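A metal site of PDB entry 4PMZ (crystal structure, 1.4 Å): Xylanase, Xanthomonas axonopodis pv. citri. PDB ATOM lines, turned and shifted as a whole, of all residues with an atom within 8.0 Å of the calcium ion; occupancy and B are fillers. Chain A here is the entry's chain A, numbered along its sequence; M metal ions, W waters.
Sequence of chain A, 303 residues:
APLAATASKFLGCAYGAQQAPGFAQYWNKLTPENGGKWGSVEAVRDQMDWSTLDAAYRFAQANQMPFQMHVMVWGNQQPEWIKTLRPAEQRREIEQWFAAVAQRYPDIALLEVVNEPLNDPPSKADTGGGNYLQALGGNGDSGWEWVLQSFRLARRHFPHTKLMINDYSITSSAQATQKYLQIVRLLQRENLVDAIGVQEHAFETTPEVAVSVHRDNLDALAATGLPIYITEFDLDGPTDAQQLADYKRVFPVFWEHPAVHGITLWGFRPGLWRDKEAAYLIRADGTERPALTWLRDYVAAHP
Water W2 bridges OE1 of Glu 42 and O of Glu 93.
The guanidinium group (NE) of Arg 45 lies within salt-bridge range of the side-chain carboxylate (OE2) of Glu 93 (2.7 Å). The indole nitrogen of Trp 81 sits at hydrogen-bond distance from the backbone carbonyl oxygen of Glu 42 (2.8 Å). NE1 of Trp 38 lies within hydrogen-bond range of OE1 of Glu 42.
Of the 16 residues printed, 4 come within 4 Å of the calcium ion.
OE1 of Gln 96 binds the calcium ion (2.3 Å). OD1 of Asp 46 is bound to the calcium ion (2.4 Å). The calcium ion is bound by water W1 (2.4 Å). OE1 of Glu 93 is bound to the calcium ion (2.4 Å). Water W2 is bound to the calcium ion (2.4 Å). The calcium ion is bound by OE2 of Glu 42.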
ATOM      1  N   TRP A  38      -8.592  34.776   5.115  1.00  0.00           N
ATOM      2  CA  TRP A  38      -8.648  33.889   6.271  1.00  0.00           C
ATOM      3  C   TRP A  38      -7.732  34.353   7.420  1.00  0.00           C
ATOM      4  O   TRP A  38      -8.124  34.320   8.581  1.00  0.00           O
ATOM      5  CB  TRP A  38      -8.344  32.449   5.863  1.00  0.00           C
ATOM      6  CG  TRP A  38      -8.706  31.400   6.884  1.00  0.00           C
ATOM      7  CD1 TRP A  38      -9.382  31.576   8.051  1.00  0.00           C
ATOM      8  CD2 TRP A  38      -8.424  29.999   6.787  1.00  0.00           C
ATOM      9  NE1 TRP A  38      -9.526  30.375   8.706  1.00  0.00           N
ATOM     10  CE2 TRP A  38      -8.956  29.390   7.952  1.00  0.00           C
ATOM     11  CE3 TRP A  38      -7.779  29.203   5.832  1.00  0.00           C
ATOM     12  CZ2 TRP A  38      -8.857  28.014   8.185  1.00  0.00           C
ATOM     13  CZ3 TRP A  38      -7.676  27.835   6.070  1.00  0.00           C
ATOM     14  CH2 TRP A  38      -8.214  27.253   7.238  1.00  0.00           C
ATOM     15  N   GLU A  42      -9.043  34.791  11.251  1.00  0.00           N
ATOM     16  CA  GLU A  42      -8.607  33.800  12.221  1.00  0.00           C
ATOM     17  C   GLU A  42      -7.088  33.787  12.369  1.00  0.00           C
ATOM     18  O   GLU A  42      -6.432  32.754  12.191  1.00  0.00           O
ATOM     19  CB  GLU A  42      -9.135  32.416  11.828  1.00  0.00           C
ATOM     20  CG  GLU A  42      -9.161  31.413  12.973  1.00  0.00           C
ATOM     21  CD  GLU A  42      -9.797  30.084  12.598  1.00  0.00           C
ATOM     22  OE1 GLU A  42     -10.258  29.904  11.456  1.00  0.00           O
ATOM     23  OE2 GLU A  42      -9.845  29.199  13.485  1.00  0.00           O
ATOM     24  N   VAL A  44      -5.570  34.089  15.119  1.00  0.00           N
ATOM     25  CA  VAL A  44      -5.378  33.172  16.240  1.00  0.00           C
ATOM     26  C   VAL A  44      -6.417  32.059  16.113  1.00  0.00           C
ATOM     27  O   VAL A  44      -7.610  32.331  15.914  1.00  0.00           O
ATOM     28  CB  VAL A  44      -5.516  33.894  17.603  1.00  0.00           C
ATOM     29  CG1 VAL A  44      -5.357  32.935  18.763  1.00  0.00           C
ATOM     30  CG2 VAL A  44      -4.490  35.029  17.712  1.00  0.00           C
ATOM     31  N   ARG A  45      -5.953  30.811  16.191  1.00  0.00           N
ATOM     32  CA  ARG A  45      -6.796  29.643  15.972  1.00  0.00           C
ATOM     33  C   ARG A  45      -8.037  29.630  16.859  1.00  0.00           C
ATOM     34  O   ARG A  45      -7.947  29.830  18.075  1.00  0.00           O
ATOM     35  CB  ARG A  45      -5.999  28.361  16.174  1.00  0.00           C
ATOM     36  CG  ARG A  45      -6.712  27.101  15.710  1.00  0.00           C
ATOM     37  CD  ARG A  45      -5.976  25.859  16.161  1.00  0.00           C
ATOM     38  NE  ARG A  45      -6.484  24.679  15.479  1.00  0.00           N
ATOM     39  CZ  ARG A  45      -5.951  23.457  15.586  1.00  0.00           C
ATOM     40  NH1 ARG A  45      -4.895  23.260  16.351  1.00  0.00           N
ATOM     41  NH2 ARG A  45      -6.480  22.447  14.912  1.00  0.00           N
ATOM     42  N   ASP A  46      -9.191  29.410  16.214  1.00  0.00           N
ATOM     43  CA  ASP A  46     -10.492  29.262  16.876  1.00  0.00           C
ATOM     44  C   ASP A  46     -11.019  30.483  17.636  1.00  0.00           C
ATOM     45  O   ASP A  46     -11.886  30.370  18.494  1.00  0.00           O
ATOM     46  CB  ASP A  46     -10.541  27.994  17.746  1.00  0.00           C
ATOM     47  CG  ASP A  46     -10.429  26.716  16.927  1.00  0.00           C
ATOM     48  OD1 ASP A  46     -10.799  26.732  15.723  1.00  0.00           O
ATOM     49  OD2 ASP A  46      -9.980  25.691  17.481  1.00  0.00           O
ATOM     50  N   GLN A  47     -10.493  31.655  17.290  1.00  0.00           N
ATOM     51  CA  GLN A  47     -11.165  32.904  17.622  1.00  0.00           C
ATOM     52  C   GLN A  47     -11.310  33.741  16.364  1.00  0.00           C
ATOM     53  O   GLN A  47     -10.322  34.031  15.674  1.00  0.00           O
ATOM     54  CB  GLN A  47     -10.490  33.658  18.786  1.00  0.00           C
ATOM     55  CG  GLN A  47      -9.067  34.123  18.547  1.00  0.00           C
ATOM     56  CD  GLN A  47      -8.428  34.680  19.809  1.00  0.00           C
ATOM     57  OE1 GLN A  47      -8.440  34.042  20.864  1.00  0.00           O
ATOM     58  NE2 GLN A  47      -7.874  35.890  19.710  1.00  0.00           N
ATOM     59  N   MET A  48     -12.548  34.094  16.041  1.00  0.00           N
ATOM     60  CA  MET A  48     -12.845  34.760  14.784  1.00  0.00           C
ATOM     61  C   MET A  48     -13.037  36.250  15.005  1.00  0.00           C
ATOM     62  O   MET A  48     -13.898  36.668  15.779  1.00  0.00           O
ATOM     63  CB  MET A  48     -14.093  34.142  14.131  1.00  0.00           C
ATOM     64  CG  MET A  48     -14.085  32.630  14.057  1.00  0.00           C
ATOM     65  SD  MET A  48     -12.754  31.950  13.051  1.00  0.00           S
ATOM     66  CE  MET A  48     -13.583  31.694  11.481  1.00  0.00           C
ATOM     67  N   TRP A  81      -0.927  29.639  12.105  1.00  0.00           N
ATOM     68  CA  TRP A  81      -1.013  28.421  12.916  1.00  0.00           C
ATOM     69  C   TRP A  81      -1.340  27.166  12.110  1.00  0.00           C
ATOM     70  O   TRP A  81      -1.078  26.043  12.560  1.00  0.00           O
ATOM     71  CB  TRP A  81      -2.031  28.603  14.055  1.00  0.00           C
ATOM     72  CG  TRP A  81      -3.349  29.121  13.575  1.00  0.00           C
ATOM     73  CD1 TRP A  81      -3.776  30.423  13.576  1.00  0.00           C
ATOM     74  CD2 TRP A  81      -4.419  28.356  12.993  1.00  0.00           C
ATOM     75  NE1 TRP A  81      -5.034  30.508  13.049  1.00  0.00           N
ATOM     76  CE2 TRP A  81      -5.454  29.261  12.674  1.00  0.00           C
ATOM     77  CE3 TRP A  81      -4.593  26.986  12.717  1.00  0.00           C
ATOM     78  CZ2 TRP A  81      -6.655  28.841  12.088  1.00  0.00           C
ATOM     79  CZ3 TRP A  81      -5.783  26.576  12.129  1.00  0.00           C
ATOM     80  CH2 TRP A  81      -6.801  27.505  11.821  1.00  0.00           C
ATOM     81  N   GLU A  89      -6.013  17.669   9.955  1.00  0.00           N
ATOM     82  CA  GLU A  89      -6.460  18.759  10.828  1.00  0.00           C
ATOM     83  C   GLU A  89      -6.603  20.073  10.076  1.00  0.00           C
ATOM     84  O   GLU A  89      -7.524  20.841  10.343  1.00  0.00           O
ATOM     85  CB  GLU A  89      -5.557  18.918  12.058  1.00  0.00           C
ATOM     86  CG  GLU A  89      -5.521  17.715  12.998  1.00  0.00           C
ATOM     87  CD  GLU A  89      -6.874  17.353  13.598  1.00  0.00           C
ATOM     88  OE1 GLU A  89      -7.850  18.124  13.498  1.00  0.00           O
ATOM     89  OE2 GLU A  89      -6.957  16.255  14.189  1.00  0.00           O
ATOM     90  N   ARG A  92     -10.013  20.012   8.276  1.00  0.00           N
ATOM     91  CA  ARG A  92     -11.118  20.294   9.188  1.00  0.00           C
ATOM     92  C   ARG A  92     -11.231  21.792   9.469  1.00  0.00           C
ATOM     93  O   ARG A  92     -12.340  22.323   9.584  1.00  0.00           O
ATOM     94  CB  ARG A  92     -10.960  19.512  10.489  1.00  0.00           C
ATOM     95  CG  ARG A  92     -11.074  18.011  10.307  1.00  0.00           C
ATOM     96  CD  ARG A  92     -10.728  17.286  11.589  1.00  0.00           C
ATOM     97  NE  ARG A  92     -11.855  17.232  12.523  1.00  0.00           N
ATOM     98  CZ  ARG A  92     -11.739  17.067  13.837  1.00  0.00           C
ATOM     99  NH1 ARG A  92     -10.547  16.964  14.395  1.00  0.00           N
ATOM    100  NH2 ARG A  92     -12.822  17.011  14.588  1.00  0.00           N
ATOM    101  N   GLU A  93     -10.082  22.461   9.549  1.00  0.00           N
ATOM    102  CA  GLU A  93     -10.038  23.907   9.760  1.00  0.00           C
ATOM    103  C   GLU A  93     -10.562  24.653   8.532  1.00  0.00           C
ATOM    104  O   GLU A  93     -11.271  25.652   8.665  1.00  0.00           O
ATOM    105  CB  GLU A  93      -8.630  24.382  10.108  1.00  0.00           C
ATOM    106  CG  GLU A  93      -8.124  23.913  11.466  1.00  0.00           C
ATOM    107  CD  GLU A  93      -8.795  24.614  12.645  1.00  0.00           C
ATOM    108  OE1 GLU A  93      -9.589  25.561  12.447  1.00  0.00           O
ATOM    109  OE2 GLU A  93      -8.535  24.189  13.795  1.00  0.00           O
ATOM    110  N   ILE A  94     -10.212  24.177   7.345  1.00  0.00           N
ATOM    111  CA  ILE A  94     -10.708  24.755   6.102  1.00  0.00           C
ATOM    112  C   ILE A  94     -12.224  24.634   6.036  1.00  0.00           C
ATOM    113  O   ILE A  94     -12.929  25.622   5.781  1.00  0.00           O
ATOM    114  CB  ILE A  94     -10.047  24.127   4.855  1.00  0.00           C
ATOM    115  CG1 ILE A  94      -8.551  24.424   4.834  1.00  0.00           C
ATOM    116  CG2 ILE A  94     -10.688  24.658   3.575  1.00  0.00           C
ATOM    117  CD1 ILE A  94      -7.747  23.517   3.916  1.00  0.00           C
ATOM    118  N   GLU A  95     -12.735  23.428   6.274  1.00  0.00           N
ATOM    119  CA  GLU A  95     -14.180  23.177   6.258  1.00  0.00           C
ATOM    120  C   GLU A  95     -14.911  24.071   7.265  1.00  0.00           C
ATOM    121  O   GLU A  95     -15.963  24.622   6.954  1.00  0.00           O
ATOM    122  CB  GLU A  95     -14.485  21.689   6.476  1.00  0.00           C
ATOM    123  CG  GLU A  95     -15.974  21.353   6.421  1.00  0.00           C
ATOM    124  CD  GLU A  95     -16.281  20.091   5.644  1.00  0.00           C
ATOM    125  OE1 GLU A  95     -15.456  19.138   5.673  1.00  0.00           O
ATOM    126  OE2 GLU A  95     -17.340  20.039   4.988  1.00  0.00           O
ATOM    127  N   GLN A  96     -14.343  24.207   8.463  1.00  0.00           N
ATOM    128  CA  GLN A  96     -14.931  25.077   9.495  1.00  0.00           C
ATOM    129  C   GLN A  96     -14.981  26.544   9.046  1.00  0.00           C
ATOM    130  O   GLN A  96     -15.978  27.234   9.287  1.00  0.00           O
ATOM    131  CB  GLN A  96     -14.160  24.954  10.819  1.00  0.00           C
ATOM    132  CG  GLN A  96     -14.698  25.855  11.920  1.00  0.00           C
ATOM    133  CD  GLN A  96     -14.154  25.524  13.288  1.00  0.00           C
ATOM    134  OE1 GLN A  96     -12.942  25.558  13.522  1.00  0.00           O
ATOM    135  NE2 GLN A  96     -15.045  25.208  14.210  1.00  0.00           N
ATOM    136  N   TRP A  97     -13.914  26.993   8.381  1.00  0.00           N
ATOM    137  CA  TRP A  97     -13.827  28.338   7.807  1.00  0.00           C
ATOM    138  C   TRP A  97     -14.921  28.574   6.757  1.00  0.00           C
ATOM    139  O   TRP A  97     -15.585  29.613   6.776  1.00  0.00           O
ATOM    140  CB  TRP A  97     -12.394  28.540   7.269  1.00  0.00           C
ATOM    141  CG  TRP A  97     -12.145  29.625   6.241  1.00  0.00           C
ATOM    142  CD1 TRP A  97     -11.611  29.444   4.998  1.00  0.00           C
ATOM    143  CD2 TRP A  97     -12.358  31.033   6.388  1.00  0.00           C
ATOM    144  NE1 TRP A  97     -11.483  30.653   4.361  1.00  0.00           N
ATOM    145  CE2 TRP A  97     -11.934  31.647   5.183  1.00  0.00           C
ATOM    146  CE3 TRP A  97     -12.864  31.848   7.421  1.00  0.00           C
ATOM    147  CZ2 TRP A  97     -12.025  33.029   4.973  1.00  0.00           C
ATOM    148  CZ3 TRP A  97     -12.938  33.232   7.213  1.00  0.00           C
ATOM    149  CH2 TRP A  97     -12.516  33.804   5.993  1.00  0.00           C
ATOM    150  N   ALA A 100     -18.315  28.646   8.596  1.00  0.00           N
ATOM    151  CA  ALA A 100     -18.427  29.894   9.365  1.00  0.00           C
ATOM    152  C   ALA A 100     -18.851  31.063   8.492  1.00  0.00           C
ATOM    153  O   ALA A 100     -19.763  31.814   8.844  1.00  0.00           O
ATOM    154  CB  ALA A 100     -17.128  30.199  10.085  1.00  0.00           C
HETATM  155 CA    CA M   1     -11.177  27.099  13.405  1.00  0.00          CA
HETATM  156  O   HOH W   1     -12.829  28.745  13.953  1.00  0.00           O
HETATM  157  O   HOH W   2     -11.564  27.370  11.021  1.00  0.00           O
